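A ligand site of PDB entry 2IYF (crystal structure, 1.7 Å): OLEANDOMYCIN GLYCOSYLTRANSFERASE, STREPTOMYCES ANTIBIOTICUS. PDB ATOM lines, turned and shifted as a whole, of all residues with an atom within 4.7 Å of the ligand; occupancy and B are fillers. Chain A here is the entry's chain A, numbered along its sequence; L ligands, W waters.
O of Trp 74 touches C25 of the ligand, 3.7 Å away.
Asn 81 touches the ligand (ND2 to C34, 3.3 Å).
CG1 of Val 82 touches O2 of the ligand, at 3.7 Å.
Phe 85 touches the ligand.
Ile 112 touches the ligand (CD1 to C16, 3.7 Å).
Tyr 115 touches the ligand (OH to C15, 3.8 Å).
Asn 134 touches the ligand (ND2 to C36, 3.4 Å).
Val 136 touches the ligand.
Ala 137 touches the ligand (N to C35, 3.8 Å).
Ala 183 touches the ligand (O to C14, 3.6 Å).
Asp 330 touches the ligand.
Hydrophobic or aromatic side chains within 4 Å of the ligand: His 20, Trp 74, Val 82, Phe 85, Ile 112 and Ala 183.
Within 4 Å of the ligand: His 20, Trp 74, Asn 81, Val 82, Phe 85, Ile 112, Tyr 115, Asn 134, Val 136, Ala 137, Ala 183, Ser 184 and Asp 330.
The guanidinium group of Arg 118 lies within hydrogen-bond range of the backbone carbonyl oxygen of Ile 112 (2.8 Å).
The side-chain amide oxygen (OD1) of Asn 81 lies close to the backbone carbonyl oxygen (O) of Trp 74 (3.1 Å).
O of Ala 183 sits at hydrogen-bond distance from NH2 of Arg 118.
An oxygen (O10) of the ligand is in hydrogen-bond range of a ring nitrogen (NE2) of His 20.
The side-chain hydroxyl (OG) of Ser 184 sits at hydrogen-bond distance from an oxygen (O7) of the ligand (2.9 Å).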
ATOM      1  N   ILE A  15       9.143  -9.979  10.380  1.00  0.00           N
ATOM      2  CA  ILE A  15       7.766  -9.563  10.508  1.00  0.00           C
ATOM      3  C   ILE A  15       7.738  -8.440  11.531  1.00  0.00           C
ATOM      4  O   ILE A  15       8.733  -8.212  12.237  1.00  0.00           O
ATOM      5  CB  ILE A  15       6.852 -10.743  10.968  1.00  0.00           C
ATOM      6  CG1 ILE A  15       7.258 -11.280  12.356  1.00  0.00           C
ATOM      7  CG2 ILE A  15       6.910 -11.917   9.926  1.00  0.00           C
ATOM      8  CD1 ILE A  15       6.144 -12.127  13.014  1.00  0.00           C
ATOM      9  N   ALA A  17       6.974  -7.795  14.589  1.00  0.00           N
ATOM     10  CA  ALA A  17       6.758  -8.235  15.961  1.00  0.00           C
ATOM     11  C   ALA A  17       8.022  -7.979  16.728  1.00  0.00           C
ATOM     12  O   ALA A  17       9.120  -8.352  16.278  1.00  0.00           O
ATOM     13  CB  ALA A  17       6.348  -9.751  16.032  1.00  0.00           C
ATOM     14  N   HIS A  20      10.602 -10.723  17.246  1.00  0.00           N
ATOM     15  CA  HIS A  20      11.259 -11.201  16.033  1.00  0.00           C
ATOM     16  C   HIS A  20      12.119 -10.149  15.325  1.00  0.00           C
ATOM     17  O   HIS A  20      12.671 -10.406  14.266  1.00  0.00           O
ATOM     18  CB  HIS A  20      10.238 -11.858  15.070  1.00  0.00           C
ATOM     19  CG  HIS A  20       9.609 -13.069  15.672  1.00  0.00           C
ATOM     20  ND1 HIS A  20      10.240 -14.290  15.751  1.00  0.00           N
ATOM     21  CD2 HIS A  20       8.423 -13.227  16.314  1.00  0.00           C
ATOM     22  CE1 HIS A  20       9.473 -15.147  16.385  1.00  0.00           C
ATOM     23  NE2 HIS A  20       8.357 -14.536  16.733  1.00  0.00           N
ATOM     24  N   TRP A  74      -2.767 -13.870  18.149  1.00  0.00           N
ATOM     25  CA  TRP A  74      -1.924 -14.866  17.429  1.00  0.00           C
ATOM     26  C   TRP A  74      -2.452 -16.300  17.492  1.00  0.00           C
ATOM     27  O   TRP A  74      -1.818 -17.238  16.984  1.00  0.00           O
ATOM     28  CB  TRP A  74      -0.483 -14.781  17.932  1.00  0.00           C
ATOM     29  CG  TRP A  74       0.179 -13.437  17.630  1.00  0.00           C
ATOM     30  CD1 TRP A  74       0.085 -12.266  18.375  1.00  0.00           C
ATOM     31  CD2 TRP A  74       1.026 -13.130  16.506  1.00  0.00           C
ATOM     32  NE1 TRP A  74       0.812 -11.269  17.771  1.00  0.00           N
ATOM     33  CE2 TRP A  74       1.394 -11.759  16.631  1.00  0.00           C
ATOM     34  CE3 TRP A  74       1.514 -13.873  15.413  1.00  0.00           C
ATOM     35  CZ2 TRP A  74       2.231 -11.113  15.699  1.00  0.00           C
ATOM     36  CZ3 TRP A  74       2.353 -13.214  14.487  1.00  0.00           C
ATOM     37  CH2 TRP A  74       2.707 -11.861  14.641  1.00  0.00           C
ATOM     38  N   ASN A  81      -2.178 -21.011  15.610  1.00  0.00           N
ATOM     39  CA  ASN A  81      -0.823 -20.480  15.739  1.00  0.00           C
ATOM     40  C   ASN A  81      -0.055 -20.543  14.400  1.00  0.00           C
ATOM     41  O   ASN A  81       0.584 -19.557  14.020  1.00  0.00           O
ATOM     42  CB  ASN A  81      -0.007 -21.212  16.807  1.00  0.00           C
ATOM     43  CG  ASN A  81      -0.470 -20.912  18.213  1.00  0.00           C
ATOM     44  OD1 ASN A  81      -1.149 -19.891  18.465  1.00  0.00           O
ATOM     45  ND2 ASN A  81      -0.154 -21.807  19.122  1.00  0.00           N
ATOM     46  N   VAL A  82      -0.069 -21.702  13.737  1.00  0.00           N
ATOM     47  CA  VAL A  82       0.819 -21.881  12.560  1.00  0.00           C
ATOM     48  C   VAL A  82       0.218 -21.415  11.241  1.00  0.00           C
ATOM     49  O   VAL A  82       0.932 -20.895  10.377  1.00  0.00           O
ATOM     50  CB  VAL A  82       1.339 -23.336  12.405  1.00  0.00           C
ATOM     51  CG1 VAL A  82       2.069 -23.746  13.656  1.00  0.00           C
ATOM     52  CG2 VAL A  82       0.200 -24.315  12.089  1.00  0.00           C
ATOM     53  N   PHE A  85       1.133 -17.936   9.549  1.00  0.00           N
ATOM     54  CA  PHE A  85       2.467 -17.727   8.957  1.00  0.00           C
ATOM     55  C   PHE A  85       2.512 -18.209   7.519  1.00  0.00           C
ATOM     56  O   PHE A  85       3.226 -17.616   6.700  1.00  0.00           O
ATOM     57  CB  PHE A  85       3.527 -18.384   9.796  1.00  0.00           C
ATOM     58  CG  PHE A  85       3.685 -17.727  11.131  1.00  0.00           C
ATOM     59  CD1 PHE A  85       3.077 -18.278  12.257  1.00  0.00           C
ATOM     60  CD2 PHE A  85       4.385 -16.522  11.244  1.00  0.00           C
ATOM     61  CE1 PHE A  85       3.200 -17.635  13.528  1.00  0.00           C
ATOM     62  CE2 PHE A  85       4.526 -15.882  12.497  1.00  0.00           C
ATOM     63  CZ  PHE A  85       3.928 -16.448  13.636  1.00  0.00           C
ATOM     64  N   ILE A 112      13.093 -16.664  12.020  1.00  0.00           N
ATOM     65  CA  ILE A 112      12.363 -17.919  11.836  1.00  0.00           C
ATOM     66  C   ILE A 112      10.960 -17.818  11.226  1.00  0.00           C
ATOM     67  O   ILE A 112      10.505 -18.775  10.601  1.00  0.00           O
ATOM     68  CB  ILE A 112      12.332 -18.755  13.167  1.00  0.00           C
ATOM     69  CG1 ILE A 112      11.735 -17.948  14.332  1.00  0.00           C
ATOM     70  CG2 ILE A 112      13.740 -19.259  13.500  1.00  0.00           C
ATOM     71  CD1 ILE A 112      11.354 -18.802  15.549  1.00  0.00           C
ATOM     72  N   THR A 113      10.280 -16.693  11.413  1.00  0.00           N
ATOM     73  CA  THR A 113       8.880 -16.568  10.984  1.00  0.00           C
ATOM     74  C   THR A 113       8.715 -16.281   9.481  1.00  0.00           C
ATOM     75  O   THR A 113       7.604 -16.373   8.972  1.00  0.00           O
ATOM     76  CB  THR A 113       8.099 -15.464  11.758  1.00  0.00           C
ATOM     77  OG1 THR A 113       8.733 -14.221  11.543  1.00  0.00           O
ATOM     78  CG2 THR A 113       8.109 -15.769  13.286  1.00  0.00           C
ATOM     79  N   TYR A 115       8.794 -17.343   6.029  1.00  0.00           N
ATOM     80  CA  TYR A 115       8.848 -18.368   4.965  1.00  0.00           C
ATOM     81  C   TYR A 115       9.295 -17.768   3.612  1.00  0.00           C
ATOM     82  O   TYR A 115      10.049 -18.439   2.919  1.00  0.00           O
ATOM     83  CB  TYR A 115       7.513 -19.090   4.766  1.00  0.00           C
ATOM     84  CG  TYR A 115       6.982 -19.824   5.991  1.00  0.00           C
ATOM     85  CD1 TYR A 115       7.848 -20.293   6.983  1.00  0.00           C
ATOM     86  CD2 TYR A 115       5.613 -20.081   6.117  1.00  0.00           C
ATOM     87  CE1 TYR A 115       7.358 -20.973   8.119  1.00  0.00           C
ATOM     88  CE2 TYR A 115       5.125 -20.794   7.237  1.00  0.00           C
ATOM     89  CZ  TYR A 115       6.003 -21.229   8.218  1.00  0.00           C
ATOM     90  OH  TYR A 115       5.516 -21.894   9.315  1.00  0.00           O
ATOM     91  N   ARG A 118      13.052 -17.942   3.061  1.00  0.00           N
ATOM     92  CA  ARG A 118      13.526 -19.290   2.740  1.00  0.00           C
ATOM     93  C   ARG A 118      13.324 -19.562   1.254  1.00  0.00           C
ATOM     94  O   ARG A 118      14.249 -20.046   0.575  1.00  0.00           O
ATOM     95  CB  ARG A 118      12.712 -20.312   3.528  1.00  0.00           C
ATOM     96  CG  ARG A 118      12.940 -20.253   5.069  1.00  0.00           C
ATOM     97  CD  ARG A 118      11.896 -21.225   5.650  1.00  0.00           C
ATOM     98  NE  ARG A 118      11.808 -21.498   7.095  1.00  0.00           N
ATOM     99  CZ  ARG A 118      11.439 -20.647   8.056  1.00  0.00           C
ATOM    100  NH1 ARG A 118      11.295 -19.355   7.825  1.00  0.00           N
ATOM    101  NH2 ARG A 118      11.302 -21.122   9.299  1.00  0.00           N
ATOM    102  N   ASN A 134      14.699 -17.882  19.992  1.00  0.00           N
ATOM    103  CA  ASN A 134      14.257 -18.860  21.011  1.00  0.00           C
ATOM    104  C   ASN A 134      14.912 -20.194  20.702  1.00  0.00           C
ATOM    105  O   ASN A 134      15.757 -20.318  19.779  1.00  0.00           O
ATOM    106  CB  ASN A 134      12.735 -19.023  20.963  1.00  0.00           C
ATOM    107  CG  ASN A 134      12.212 -19.177  19.530  1.00  0.00           C
ATOM    108  OD1 ASN A 134      12.365 -20.240  18.875  1.00  0.00           O
ATOM    109  ND2 ASN A 134      11.633 -18.102  19.040  1.00  0.00           N
ATOM    110  N   LEU A 135      14.543 -21.191  21.499  1.00  0.00           N
ATOM    111  CA  LEU A 135      15.103 -22.550  21.319  1.00  0.00           C
ATOM    112  C   LEU A 135      14.866 -23.083  19.881  1.00  0.00           C
ATOM    113  O   LEU A 135      13.914 -22.667  19.174  1.00  0.00           O
ATOM    114  CB  LEU A 135      14.553 -23.515  22.398  1.00  0.00           C
ATOM    115  CG  LEU A 135      13.027 -23.677  22.260  1.00  0.00           C
ATOM    116  CD1 LEU A 135      12.679 -24.903  21.446  1.00  0.00           C
ATOM    117  CD2 LEU A 135      12.419 -23.787  23.679  1.00  0.00           C
ATOM    118  N   VAL A 136      15.738 -24.010  19.504  1.00  0.00           N
ATOM    119  CA  VAL A 136      15.667 -24.649  18.186  1.00  0.00           C
ATOM    120  C   VAL A 136      15.474 -26.169  18.341  1.00  0.00           C
ATOM    121  O   VAL A 136      15.580 -26.734  19.438  1.00  0.00           O
ATOM    122  CB  VAL A 136      16.971 -24.393  17.362  1.00  0.00           C
ATOM    123  CG1 VAL A 136      17.124 -22.916  17.029  1.00  0.00           C
ATOM    124  CG2 VAL A 136      18.198 -24.944  18.112  1.00  0.00           C
ATOM    125  N   ALA A 137      15.194 -26.842  17.215  1.00  0.00           N
ATOM    126  CA  ALA A 137      15.139 -28.307  17.208  1.00  0.00           C
ATOM    127  C   ALA A 137      16.490 -28.962  17.534  1.00  0.00           C
ATOM    128  O   ALA A 137      17.533 -28.493  17.087  1.00  0.00           O
ATOM    129  CB  ALA A 137      14.651 -28.794  15.818  1.00  0.00           C
ATOM    130  N   TYR A 141      13.990 -34.211  17.811  1.00  0.00           N
ATOM    131  CA  TYR A 141      12.826 -33.333  17.978  1.00  0.00           C
ATOM    132  C   TYR A 141      11.629 -33.821  17.153  1.00  0.00           C
ATOM    133  O   TYR A 141      10.491 -33.730  17.588  1.00  0.00           O
ATOM    134  CB  TYR A 141      13.194 -31.903  17.573  1.00  0.00           C
ATOM    135  CG  TYR A 141      12.012 -30.954  17.447  1.00  0.00           C
ATOM    136  CD1 TYR A 141      11.427 -30.721  16.198  1.00  0.00           C
ATOM    137  CD2 TYR A 141      11.518 -30.251  18.546  1.00  0.00           C
ATOM    138  CE1 TYR A 141      10.354 -29.872  16.053  1.00  0.00           C
ATOM    139  CE2 TYR A 141      10.425 -29.361  18.402  1.00  0.00           C
ATOM    140  CZ  TYR A 141       9.862 -29.184  17.133  1.00  0.00           C
ATOM    141  OH  TYR A 141       8.798 -28.337  16.915  1.00  0.00           O
ATOM    142  N   ALA A 183      10.111 -25.587   7.334  1.00  0.00           N
ATOM    143  CA  ALA A 183       9.781 -24.656   8.422  1.00  0.00           C
ATOM    144  C   ALA A 183      10.710 -24.785   9.654  1.00  0.00           C
ATOM    145  O   ALA A 183      11.169 -23.759  10.186  1.00  0.00           O
ATOM    146  CB  ALA A 183       8.304 -24.797   8.826  1.00  0.00           C
ATOM    147  N   SER A 184      10.994 -26.015  10.079  1.00  0.00           N
ATOM    148  CA  SER A 184      11.591 -26.225  11.414  1.00  0.00           C
ATOM    149  C   SER A 184      13.051 -26.626  11.370  1.00  0.00           C
ATOM    150  O   SER A 184      13.673 -26.724  12.431  1.00  0.00           O
ATOM    151  CB  SER A 184      10.828 -27.281  12.228  1.00  0.00           C
ATOM    152  OG  SER A 184       9.452 -26.909  12.462  1.00  0.00           O
ATOM    153  N   ASP A 330       5.064 -19.320  28.245  1.00  0.00           N
ATOM    154  CA  ASP A 330       6.411 -19.121  27.747  1.00  0.00           C
ATOM    155  C   ASP A 330       7.539 -19.080  28.818  1.00  0.00           C
ATOM    156  O   ASP A 330       8.705 -18.913  28.459  1.00  0.00           O
ATOM    157  CB  ASP A 330       6.451 -17.858  26.871  1.00  0.00           C
ATOM    158  CG  ASP A 330       5.389 -16.828  27.270  1.00  0.00           C
ATOM    159  OD1 ASP A 330       5.493 -16.270  28.382  1.00  0.00           O
ATOM    160  OD2 ASP A 330       4.461 -16.556  26.456  1.00  0.00           O
HETATM  161  C1  LIG L   1       7.924 -22.334  13.379  1.00  0.00           C
HETATM  162  C2  LIG L   1       8.355 -23.282  14.504  1.00  0.00           C
HETATM  163  C3  LIG L   1       9.884 -23.553  14.682  1.00  0.00           C
HETATM  164  C4  LIG L   1      10.141 -24.177  16.072  1.00  0.00           C
HETATM  165  O1  LIG L   1      10.051 -23.096  17.013  1.00  0.00           O
HETATM  166  C5  LIG L   1       9.054 -21.941  18.872  1.00  0.00           C
HETATM  167  C6  LIG L   1       7.670 -21.286  18.761  1.00  0.00           C
HETATM  168  C7  LIG L   1       7.642 -20.172  17.710  1.00  0.00           C
HETATM  169  C8  LIG L   1       6.162 -19.813  17.343  1.00  0.00           C
HETATM  170  C9  LIG L   1       5.677 -20.487  16.048  1.00  0.00           C
HETATM  171  C10 LIG L   1       6.439 -19.910  14.845  1.00  0.00           C
HETATM  172  C11 LIG L   1       6.019 -20.564  13.518  1.00  0.00           C
HETATM  173  C12 LIG L   1       6.446 -22.004  13.396  1.00  0.00           C
HETATM  174  O2  LIG L   1       5.613 -22.918  13.261  1.00  0.00           O
HETATM  175  C13 LIG L   1       9.077 -23.174  18.040  1.00  0.00           C
HETATM  176  O3  LIG L   1       8.345 -24.147  18.179  1.00  0.00           O
HETATM  177  O4  LIG L   1       7.254 -20.775  20.034  1.00  0.00           O
HETATM  178  O5  LIG L   1       6.099 -18.422  17.180  1.00  0.00           O
HETATM  179  C14 LIG L   1       8.198 -22.877  11.973  1.00  0.00           C
HETATM  180  C15 LIG L   1       6.570 -19.762  12.330  1.00  0.00           C
HETATM  181  C16 LIG L   1      10.706 -22.289  14.479  1.00  0.00           C
HETATM  182  O6  LIG L   1       7.633 -24.519  14.348  1.00  0.00           O
HETATM  183  O7  LIG L   1      10.314 -24.420  13.628  1.00  0.00           O
HETATM  184  C17 LIG L   1      11.543 -24.767  16.242  1.00  0.00           C
HETATM  185  C18 LIG L   1       9.558 -22.391  20.261  1.00  0.00           C
HETATM  186  C19 LIG L   1       4.144 -20.452  15.900  1.00  0.00           C
HETATM  187  O8  LIG L   1       6.042 -21.858  16.135  1.00  0.00           O
HETATM  188  C20 LIG L   1       5.281 -17.720  18.132  1.00  0.00           C
HETATM  189  C21 LIG L   1       5.543 -16.208  18.011  1.00  0.00           C
HETATM  190  C22 LIG L   1       4.539 -15.442  18.876  1.00  0.00           C
HETATM  191  C23 LIG L   1       3.096 -15.895  18.569  1.00  0.00           C
HETATM  192  C24 LIG L   1       2.953 -17.425  18.694  1.00  0.00           C
HETATM  193  O9  LIG L   1       3.926 -18.043  17.837  1.00  0.00           O
HETATM  194  N1  LIG L   1       4.563 -13.986  18.581  1.00  0.00           N
HETATM  195  C25 LIG L   1       1.600 -17.885  18.188  1.00  0.00           C
HETATM  196  O10 LIG L   1       6.859 -15.906  18.500  1.00  0.00           O
HETATM  197  C26 LIG L   1       4.100 -13.095  19.644  1.00  0.00           C
HETATM  198  C27 LIG L   1       6.479 -21.718  20.824  1.00  0.00           C
HETATM  199  C28 LIG L   1       6.584 -21.329  22.301  1.00  0.00           C
HETATM  200  C29 LIG L   1       5.723 -20.116  22.693  1.00  0.00           C
HETATM  201  C30 LIG L   1       4.268 -20.365  22.256  1.00  0.00           C
HETATM  202  C31 LIG L   1       4.262 -20.684  20.760  1.00  0.00           C
HETATM  203  O11 LIG L   1       5.115 -21.795  20.405  1.00  0.00           O
HETATM  204  O12 LIG L   1       6.162 -18.919  22.024  1.00  0.00           O
HETATM  205  O13 LIG L   1       3.527 -19.152  22.455  1.00  0.00           O
HETATM  206  C32 LIG L   1       7.446 -18.275  22.203  1.00  0.00           C
HETATM  207  C33 LIG L   1       4.814 -13.450  17.243  1.00  0.00           C
HETATM  208  C34 LIG L   1       2.865 -21.094  20.279  1.00  0.00           C
HETATM  209  C35 LIG L   1      11.647 -25.555  17.523  1.00  0.00           C
HETATM  210  C36 LIG L   1       8.452 -18.971  18.221  1.00  0.00           C
HETATM  211  C37 LIG L   1       5.734 -19.869  24.212  1.00  0.00           C
HETATM  212  O   HOH W   1       5.311 -25.401  16.211  1.00  0.00           O
HETATM  213  O   HOH W   2       2.139 -19.716  25.162  1.00  0.00           O
HETATM  214  O   HOH W   3       4.441 -23.489  17.823  1.00  0.00           O
HETATM  215  O   HOH W   4       5.254 -25.505  12.157  1.00  0.00           O
HETATM  216  O   HOH W   5       7.206 -12.673  19.745  1.00  0.00           O
HETATM  217  O   HOH W   6       4.525 -16.527  22.303  1.00  0.00           O
